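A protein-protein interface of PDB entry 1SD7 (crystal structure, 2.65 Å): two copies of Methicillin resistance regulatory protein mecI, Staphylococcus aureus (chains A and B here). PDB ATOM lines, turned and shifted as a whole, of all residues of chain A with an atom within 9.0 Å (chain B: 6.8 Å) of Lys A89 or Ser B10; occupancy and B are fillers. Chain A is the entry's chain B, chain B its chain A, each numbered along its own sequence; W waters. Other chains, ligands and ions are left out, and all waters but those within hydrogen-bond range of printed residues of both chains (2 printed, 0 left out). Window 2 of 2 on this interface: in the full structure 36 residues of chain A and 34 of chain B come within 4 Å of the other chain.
ND2 of Asn B17 is in hydrogen-bond range of O of Val A90, at 3.3 Å.
The backbone carbonyl oxygen of Trp B13 lies within hydrogen-bond range of the side-chain amide nitrogen of Asn B17, at 3.2 Å.
Among the printed residues, merely in contact across the chains: Phe A86 with Thr B82, Lys A89 with Ser B10, Lys A89 with Trp B13, Lys A89 with Asn B17, Val A90 with Trp B13 and Lys A92 with Asn B17.
Lys A89 touches just these residues of chain B: Ser B10, Trp B13 and Asn B17. Ser B10 touches just one residue of chain A: Lys A89 (3.7 Å). No residue of chain A comes within 4 Å of Ser B9. No residue of chain A comes within 4 Å of Ala B11. Printed residues of chain A within 4 Å of Trp B13: Lys A89 and Val A90. Of the printed residues of chain A, Thr B82 touches Phe A86. Ile B8 touches none of the printed residues of chain A. The nearest printed residue of chain A that does not touch Asn B17 is Tyr A91 (5.0 Å).
Hydrophobic or aromatic side chains of chain B that line the printed part of chain A: Trp B13. Of the 13 printed residues of chain A, 4 touch a printed residue of chain B. Printed residues of chain A that touch a printed residue of chain B: Phe A86, Lys A89, Val A90 and Lys A92. Hydrophobic or aromatic side chains of chain A that line the printed part of chain B: Phe A86 and Val A90. Along chain A the printed residues that touch a printed residue of chain B span positions 86 to 92. Among the printed residues, no Asp or Glu carboxylate lies within 4 Å of a Lys or Arg side-chain nitrogen of the other chain.
1 position is printed for both chains.
Water W1 bridges the side-chain amino group (NZ) of Lys A89 (2.5 Å) and the backbone carbonyl oxygen (O) of Ile B8 (3.1 Å). Water W2 lies within hydrogen-bond range of O of Asn A88 (3.2 Å) and OE2 of Glu B14 (3.3 Å).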
ATOM      1  N   GLU A   7      -4.456 -19.186  -0.452  1.00  0.00           N
ATOM      2  CA  GLU A   7      -3.949 -20.315   0.330  1.00  0.00           C
ATOM      3  C   GLU A   7      -3.808 -21.640  -0.435  1.00  0.00           C
ATOM      4  O   GLU A   7      -4.773 -22.355  -0.665  1.00  0.00           O
ATOM      5  CB  GLU A   7      -4.794 -20.485   1.600  1.00  0.00           C
ATOM      6  CG  GLU A   7      -4.748 -19.257   2.573  1.00  0.00           C
ATOM      7  CD  GLU A   7      -3.398 -19.077   3.305  1.00  0.00           C
ATOM      8  OE1 GLU A   7      -2.990 -20.005   4.036  1.00  0.00           O
ATOM      9  OE2 GLU A   7      -2.748 -18.009   3.163  1.00  0.00           O
ATOM     10  N   THR A  82       1.495 -15.483   3.322  1.00  0.00           N
ATOM     11  CA  THR A  82       1.250 -16.790   3.878  1.00  0.00           C
ATOM     12  C   THR A  82       1.701 -16.822   5.356  1.00  0.00           C
ATOM     13  O   THR A  82       0.961 -17.292   6.207  1.00  0.00           O
ATOM     14  CB  THR A  82       1.992 -17.848   3.040  1.00  0.00           C
ATOM     15  OG1 THR A  82       1.599 -17.725   1.668  1.00  0.00           O
ATOM     16  CG2 THR A  82       1.668 -19.265   3.524  1.00  0.00           C
ATOM     17  N   SER A  83       2.899 -16.311   5.663  1.00  0.00           N
ATOM     18  CA  SER A  83       3.407 -16.250   7.043  1.00  0.00           C
ATOM     19  C   SER A  83       2.509 -15.437   7.980  1.00  0.00           C
ATOM     20  O   SER A  83       2.304 -15.815   9.129  1.00  0.00           O
ATOM     21  CB  SER A  83       4.815 -15.669   7.068  1.00  0.00           C
ATOM     22  OG  SER A  83       5.773 -16.642   6.720  1.00  0.00           O
ATOM     23  N   LYS A  84       1.967 -14.330   7.494  1.00  0.00           N
ATOM     24  CA  LYS A  84       1.077 -13.515   8.318  1.00  0.00           C
ATOM     25  C   LYS A  84      -0.164 -14.318   8.647  1.00  0.00           C
ATOM     26  O   LYS A  84      -0.670 -14.244   9.749  1.00  0.00           O
ATOM     27  CB  LYS A  84       0.630 -12.246   7.586  1.00  0.00           C
ATOM     28  CG  LYS A  84       1.731 -11.291   7.251  1.00  0.00           C
ATOM     29  CD  LYS A  84       2.157 -10.531   8.459  1.00  0.00           C
ATOM     30  CE  LYS A  84       1.150  -9.478   8.846  1.00  0.00           C
ATOM     31  NZ  LYS A  84       1.578  -8.869  10.135  1.00  0.00           N
ATOM     32  N   ASN A  85      -0.655 -15.073   7.670  1.00  0.00           N
ATOM     33  CA  ASN A  85      -1.863 -15.863   7.867  1.00  0.00           C
ATOM     34  C   ASN A  85      -1.651 -16.998   8.854  1.00  0.00           C
ATOM     35  O   ASN A  85      -2.549 -17.313   9.640  1.00  0.00           O
ATOM     36  CB  ASN A  85      -2.395 -16.455   6.537  1.00  0.00           C
ATOM     37  CG  ASN A  85      -2.949 -15.395   5.577  1.00  0.00           C
ATOM     38  OD1 ASN A  85      -3.299 -14.286   5.981  1.00  0.00           O
ATOM     39  ND2 ASN A  85      -3.038 -15.748   4.298  1.00  0.00           N
ATOM     40  N   PHE A  86      -0.467 -17.606   8.809  1.00  0.00           N
ATOM     41  CA  PHE A  86      -0.168 -18.733   9.671  1.00  0.00           C
ATOM     42  C   PHE A  86      -0.101 -18.264  11.111  1.00  0.00           C
ATOM     43  O   PHE A  86      -0.634 -18.916  12.016  1.00  0.00           O
ATOM     44  CB  PHE A  86       1.158 -19.350   9.260  1.00  0.00           C
ATOM     45  CG  PHE A  86       1.636 -20.417  10.183  1.00  0.00           C
ATOM     46  CD1 PHE A  86       1.047 -21.675  10.176  1.00  0.00           C
ATOM     47  CD2 PHE A  86       2.652 -20.146  11.100  1.00  0.00           C
ATOM     48  CE1 PHE A  86       1.456 -22.650  11.065  1.00  0.00           C
ATOM     49  CE2 PHE A  86       3.078 -21.112  12.005  1.00  0.00           C
ATOM     50  CZ  PHE A  86       2.480 -22.370  11.991  1.00  0.00           C
ATOM     51  N   ILE A  87       0.548 -17.114  11.289  1.00  0.00           N
ATOM     52  CA  ILE A  87       0.747 -16.498  12.575  1.00  0.00           C
ATOM     53  C   ILE A  87      -0.564 -16.042  13.189  1.00  0.00           C
ATOM     54  O   ILE A  87      -0.760 -16.153  14.399  1.00  0.00           O
ATOM     55  CB  ILE A  87       1.767 -15.320  12.446  1.00  0.00           C
ATOM     56  CG1 ILE A  87       3.162 -15.880  12.150  1.00  0.00           C
ATOM     57  CG2 ILE A  87       1.786 -14.480  13.732  1.00  0.00           C
ATOM     58  CD1 ILE A  87       4.071 -14.886  11.512  1.00  0.00           C
ATOM     59  N   ASN A  88      -1.467 -15.539  12.360  1.00  0.00           N
ATOM     60  CA  ASN A  88      -2.778 -15.097  12.830  1.00  0.00           C
ATOM     61  C   ASN A  88      -3.666 -16.280  13.225  1.00  0.00           C
ATOM     62  O   ASN A  88      -4.518 -16.164  14.092  1.00  0.00           O
ATOM     63  CB  ASN A  88      -3.479 -14.297  11.749  1.00  0.00           C
ATOM     64  CG  ASN A  88      -4.853 -13.826  12.180  1.00  0.00           C
ATOM     65  OD1 ASN A  88      -5.890 -14.330  11.710  1.00  0.00           O
ATOM     66  ND2 ASN A  88      -4.875 -12.854  13.090  1.00  0.00           N
ATOM     67  N   LYS A  89      -3.452 -17.416  12.585  1.00  0.00           N
ATOM     68  CA  LYS A  89      -4.213 -18.621  12.859  1.00  0.00           C
ATOM     69  C   LYS A  89      -3.782 -19.342  14.132  1.00  0.00           C
ATOM     70  O   LYS A  89      -4.609 -19.788  14.913  1.00  0.00           O
ATOM     71  CB  LYS A  89      -4.084 -19.602  11.673  1.00  0.00           C
ATOM     72  CG  LYS A  89      -4.761 -20.924  11.926  1.00  0.00           C
ATOM     73  CD  LYS A  89      -4.603 -21.873  10.778  1.00  0.00           C
ATOM     74  CE  LYS A  89      -3.196 -22.343  10.684  1.00  0.00           C
ATOM     75  NZ  LYS A  89      -3.044 -23.393   9.675  1.00  0.00           N
ATOM     76  N   VAL A  90      -2.479 -19.449  14.327  1.00  0.00           N
ATOM     77  CA  VAL A  90      -1.919 -20.162  15.452  1.00  0.00           C
ATOM     78  C   VAL A  90      -1.518 -19.330  16.664  1.00  0.00           C
ATOM     79  O   VAL A  90      -1.799 -19.718  17.799  1.00  0.00           O
ATOM     80  CB  VAL A  90      -0.698 -20.994  14.970  1.00  0.00           C
ATOM     81  CG1 VAL A  90       0.026 -21.636  16.145  1.00  0.00           C
ATOM     82  CG2 VAL A  90      -1.171 -22.067  14.002  1.00  0.00           C
ATOM     83  N   TYR A  91      -0.891 -18.181  16.441  1.00  0.00           N
ATOM     84  CA  TYR A  91      -0.420 -17.367  17.565  1.00  0.00           C
ATOM     85  C   TYR A  91      -1.298 -16.191  17.905  1.00  0.00           C
ATOM     86  O   TYR A  91      -1.908 -15.605  17.048  1.00  0.00           O
ATOM     87  CB  TYR A  91       1.004 -16.889  17.278  1.00  0.00           C
ATOM     88  CG  TYR A  91       1.998 -18.029  17.135  1.00  0.00           C
ATOM     89  CD1 TYR A  91       2.644 -18.547  18.245  1.00  0.00           C
ATOM     90  CD2 TYR A  91       2.267 -18.605  15.892  1.00  0.00           C
ATOM     91  CE1 TYR A  91       3.528 -19.606  18.132  1.00  0.00           C
ATOM     92  CE2 TYR A  91       3.156 -19.671  15.771  1.00  0.00           C
ATOM     93  CZ  TYR A  91       3.778 -20.161  16.900  1.00  0.00           C
ATOM     94  OH  TYR A  91       4.654 -21.215  16.815  1.00  0.00           O
ATOM     95  N   LYS A  92      -1.357 -15.838  19.175  1.00  0.00           N
ATOM     96  CA  LYS A  92      -2.186 -14.723  19.594  1.00  0.00           C
ATOM     97  C   LYS A  92      -1.330 -13.481  19.641  1.00  0.00           C
ATOM     98  O   LYS A  92      -1.773 -12.400  19.255  1.00  0.00           O
ATOM     99  CB  LYS A  92      -2.793 -14.995  20.970  1.00  0.00           C
ATOM    100  CG  LYS A  92      -3.882 -16.043  20.956  1.00  0.00           C
ATOM    101  CD  LYS A  92      -3.468 -17.297  21.708  1.00  0.00           C
ATOM    102  CE  LYS A  92      -3.295 -17.045  23.201  1.00  0.00           C
ATOM    103  NZ  LYS A  92      -3.060 -18.318  23.951  1.00  0.00           N
ATOM    104  N   GLY A  94       1.845 -12.577  17.986  1.00  0.00           N
ATOM    105  CA  GLY A  94       2.157 -12.101  16.655  1.00  0.00           C
ATOM    106  C   GLY A  94       3.457 -12.777  16.280  1.00  0.00           C
ATOM    107  O   GLY A  94       3.796 -13.805  16.870  1.00  0.00           O
ATOM    108  N   ILE B   8      -4.355 -30.126  13.818  1.00  0.00           N
ATOM    109  CA  ILE B   8      -5.388 -29.075  13.840  1.00  0.00           C
ATOM    110  C   ILE B   8      -5.700 -28.190  12.624  1.00  0.00           C
ATOM    111  O   ILE B   8      -4.792 -27.775  11.915  1.00  0.00           O
ATOM    112  CB  ILE B   8      -5.073 -28.119  15.022  1.00  0.00           C
ATOM    113  CG1 ILE B   8      -4.894 -28.905  16.306  1.00  0.00           C
ATOM    114  CG2 ILE B   8      -6.154 -27.156  15.225  1.00  0.00           C
ATOM    115  CD1 ILE B   8      -4.809 -28.002  17.481  1.00  0.00           C
ATOM    116  N   SER B   9      -6.988 -27.861  12.441  1.00  0.00           N
ATOM    117  CA  SER B   9      -7.435 -26.984  11.361  1.00  0.00           C
ATOM    118  C   SER B   9      -7.562 -25.586  11.913  1.00  0.00           C
ATOM    119  O   SER B   9      -7.466 -25.348  13.111  1.00  0.00           O
ATOM    120  CB  SER B   9      -8.805 -27.369  10.821  1.00  0.00           C
ATOM    121  OG  SER B   9      -9.837 -26.956  11.711  1.00  0.00           O
ATOM    122  N   SER B  10      -7.835 -24.660  11.020  1.00  0.00           N
ATOM    123  CA  SER B  10      -7.955 -23.272  11.397  1.00  0.00           C
ATOM    124  C   SER B  10      -9.017 -22.977  12.476  1.00  0.00           C
ATOM    125  O   SER B  10      -8.810 -22.103  13.317  1.00  0.00           O
ATOM    126  CB  SER B  10      -8.212 -22.441  10.139  1.00  0.00           C
ATOM    127  OG  SER B  10      -8.235 -21.052  10.439  1.00  0.00           O
ATOM    128  N   ALA B  11     -10.138 -23.694  12.462  1.00  0.00           N
ATOM    129  CA  ALA B  11     -11.177 -23.444  13.451  1.00  0.00           C
ATOM    130  C   ALA B  11     -10.907 -24.099  14.798  1.00  0.00           C
ATOM    131  O   ALA B  11     -11.396 -23.614  15.815  1.00  0.00           O
ATOM    132  CB  ALA B  11     -12.534 -23.876  12.930  1.00  0.00           C
ATOM    133  N   GLU B  12     -10.164 -25.202  14.810  1.00  0.00           N
ATOM    134  CA  GLU B  12      -9.830 -25.857  16.072  1.00  0.00           C
ATOM    135  C   GLU B  12      -8.763 -24.995  16.746  1.00  0.00           C
ATOM    136  O   GLU B  12      -8.720 -24.898  17.975  1.00  0.00           O
ATOM    137  CB  GLU B  12      -9.309 -27.262  15.818  1.00  0.00           C
ATOM    138  CG  GLU B  12     -10.343 -28.153  15.137  1.00  0.00           C
ATOM    139  CD  GLU B  12      -9.730 -29.333  14.416  1.00  0.00           C
ATOM    140  OE1 GLU B  12     -10.195 -30.464  14.624  1.00  0.00           O
ATOM    141  OE2 GLU B  12      -8.787 -29.131  13.627  1.00  0.00           O
ATOM    142  N   TRP B  13      -7.898 -24.364  15.945  1.00  0.00           N
ATOM    143  CA  TRP B  13      -6.890 -23.486  16.514  1.00  0.00           C
ATOM    144  C   TRP B  13      -7.666 -22.377  17.237  1.00  0.00           C
ATOM    145  O   TRP B  13      -7.349 -22.004  18.369  1.00  0.00           O
ATOM    146  CB  TRP B  13      -5.983 -22.892  15.420  1.00  0.00           C
ATOM    147  CG  TRP B  13      -4.769 -23.746  15.109  1.00  0.00           C
ATOM    148  CD1 TRP B  13      -4.459 -24.341  13.909  1.00  0.00           C
ATOM    149  CD2 TRP B  13      -3.717 -24.117  16.024  1.00  0.00           C
ATOM    150  NE1 TRP B  13      -3.282 -25.052  14.029  1.00  0.00           N
ATOM    151  CE2 TRP B  13      -2.811 -24.931  15.314  1.00  0.00           C
ATOM    152  CE3 TRP B  13      -3.461 -23.837  17.372  1.00  0.00           C
ATOM    153  CZ2 TRP B  13      -1.665 -25.473  15.910  1.00  0.00           C
ATOM    154  CZ3 TRP B  13      -2.323 -24.371  17.966  1.00  0.00           C
ATOM    155  CH2 TRP B  13      -1.437 -25.184  17.233  1.00  0.00           C
ATOM    156  N   GLU B  14      -8.706 -21.871  16.596  1.00  0.00           N
ATOM    157  CA  GLU B  14      -9.513 -20.826  17.208  1.00  0.00           C
ATOM    158  C   GLU B  14     -10.005 -21.338  18.564  1.00  0.00           C
ATOM    159  O   GLU B  14      -9.599 -20.859  19.610  1.00  0.00           O
ATOM    160  CB  GLU B  14     -10.702 -20.488  16.321  1.00  0.00           C
ATOM    161  CG  GLU B  14     -11.238 -19.149  16.582  1.00  0.00           C
ATOM    162  CD  GLU B  14     -10.504 -18.107  15.813  1.00  0.00           C
ATOM    163  OE1 GLU B  14     -10.820 -16.916  16.006  1.00  0.00           O
ATOM    164  OE2 GLU B  14      -9.622 -18.474  15.010  1.00  0.00           O
ATOM    165  N   VAL B  15     -10.885 -22.321  18.531  1.00  0.00           N
ATOM    166  CA  VAL B  15     -11.404 -22.911  19.745  1.00  0.00           C
ATOM    167  C   VAL B  15     -10.299 -23.168  20.756  1.00  0.00           C
ATOM    168  O   VAL B  15     -10.397 -22.738  21.888  1.00  0.00           O
ATOM    169  CB  VAL B  15     -12.112 -24.210  19.413  1.00  0.00           C
ATOM    170  CG1 VAL B  15     -12.630 -24.877  20.686  1.00  0.00           C
ATOM    171  CG2 VAL B  15     -13.211 -23.907  18.426  1.00  0.00           C
ATOM    172  N   ASN B  17      -7.249 -21.877  21.148  1.00  0.00           N
ATOM    173  CA  ASN B  17      -6.651 -20.688  21.737  1.00  0.00           C
ATOM    174  C   ASN B  17      -7.443 -20.096  22.877  1.00  0.00           C
ATOM    175  O   ASN B  17      -6.873 -19.532  23.799  1.00  0.00           O
ATOM    176  CB  ASN B  17      -6.361 -19.635  20.675  1.00  0.00           C
ATOM    177  CG  ASN B  17      -5.018 -19.847  20.040  1.00  0.00           C
ATOM    178  OD1 ASN B  17      -4.023 -20.012  20.745  1.00  0.00           O
ATOM    179  ND2 ASN B  17      -4.971 -19.857  18.706  1.00  0.00           N
ATOM    180  N   LYS B  38     -15.956 -14.295  15.084  1.00  0.00           N
ATOM    181  CA  LYS B  38     -16.465 -14.983  13.911  1.00  0.00           C
ATOM    182  C   LYS B  38     -17.973 -15.145  13.940  1.00  0.00           C
ATOM    183  O   LYS B  38     -18.568 -15.315  14.988  1.00  0.00           O
ATOM    184  CB  LYS B  38     -15.767 -16.340  13.777  1.00  0.00           C
ATOM    185  CG  LYS B  38     -14.418 -16.403  14.515  1.00  0.00           C
ATOM    186  CD  LYS B  38     -13.276 -16.962  13.675  1.00  0.00           C
ATOM    187  CE  LYS B  38     -12.834 -15.973  12.609  1.00  0.00           C
ATOM    188  NZ  LYS B  38     -11.562 -16.398  11.956  1.00  0.00           N
ATOM    189  N   TRP B  40     -19.925 -17.539  13.298  1.00  0.00           N
ATOM    190  CA  TRP B  40     -20.210 -18.979  13.231  1.00  0.00           C
ATOM    191  C   TRP B  40     -21.347 -19.299  14.216  1.00  0.00           C
ATOM    192  O   TRP B  40     -21.401 -18.736  15.314  1.00  0.00           O
ATOM    193  CB  TRP B  40     -18.981 -19.805  13.643  1.00  0.00           C
ATOM    194  CG  TRP B  40     -17.729 -19.586  12.846  1.00  0.00           C
ATOM    195  CD1 TRP B  40     -17.612 -18.999  11.605  1.00  0.00           C
ATOM    196  CD2 TRP B  40     -16.418 -20.009  13.213  1.00  0.00           C
ATOM    197  NE1 TRP B  40     -16.300 -19.037  11.192  1.00  0.00           N
ATOM    198  CE2 TRP B  40     -15.549 -19.651  12.163  1.00  0.00           C
ATOM    199  CE3 TRP B  40     -15.894 -20.658  14.331  1.00  0.00           C
ATOM    200  CZ2 TRP B  40     -14.187 -19.915  12.202  1.00  0.00           C
ATOM    201  CZ3 TRP B  40     -14.531 -20.924  14.366  1.00  0.00           C
ATOM    202  CH2 TRP B  40     -13.695 -20.553  13.308  1.00  0.00           C
ATOM    203  N   LEU B  48     -17.168 -28.332  16.735  1.00  0.00           N
ATOM    204  CA  LEU B  48     -15.712 -28.192  16.863  1.00  0.00           C
ATOM    205  C   LEU B  48     -15.239 -28.653  18.238  1.00  0.00           C
ATOM    206  O   LEU B  48     -14.154 -29.209  18.359  1.00  0.00           O
ATOM    207  CB  LEU B  48     -15.262 -26.725  16.664  1.00  0.00           C
ATOM    208  CG  LEU B  48     -15.328 -26.124  15.257  1.00  0.00           C
ATOM    209  CD1 LEU B  48     -15.246 -24.608  15.353  1.00  0.00           C
ATOM    210  CD2 LEU B  48     -14.198 -26.682  14.387  1.00  0.00           C
ATOM    211  N   THR B  82       3.846 -27.249  15.078  1.00  0.00           N
ATOM    212  CA  THR B  82       3.109 -26.750  13.921  1.00  0.00           C
ATOM    213  C   THR B  82       3.980 -25.773  13.112  1.00  0.00           C
ATOM    214  O   THR B  82       4.009 -25.837  11.875  1.00  0.00           O
ATOM    215  CB  THR B  82       1.744 -26.112  14.345  1.00  0.00           C
ATOM    216  OG1 THR B  82       0.892 -27.137  14.872  1.00  0.00           O
ATOM    217  CG2 THR B  82       1.036 -25.454  13.153  1.00  0.00           C
HETATM  218  O   HOH W   1      -4.514 -25.440   9.940  1.00  0.00           O
HETATM  219  O   HOH W   2      -7.703 -16.002  13.947  1.00  0.00           O
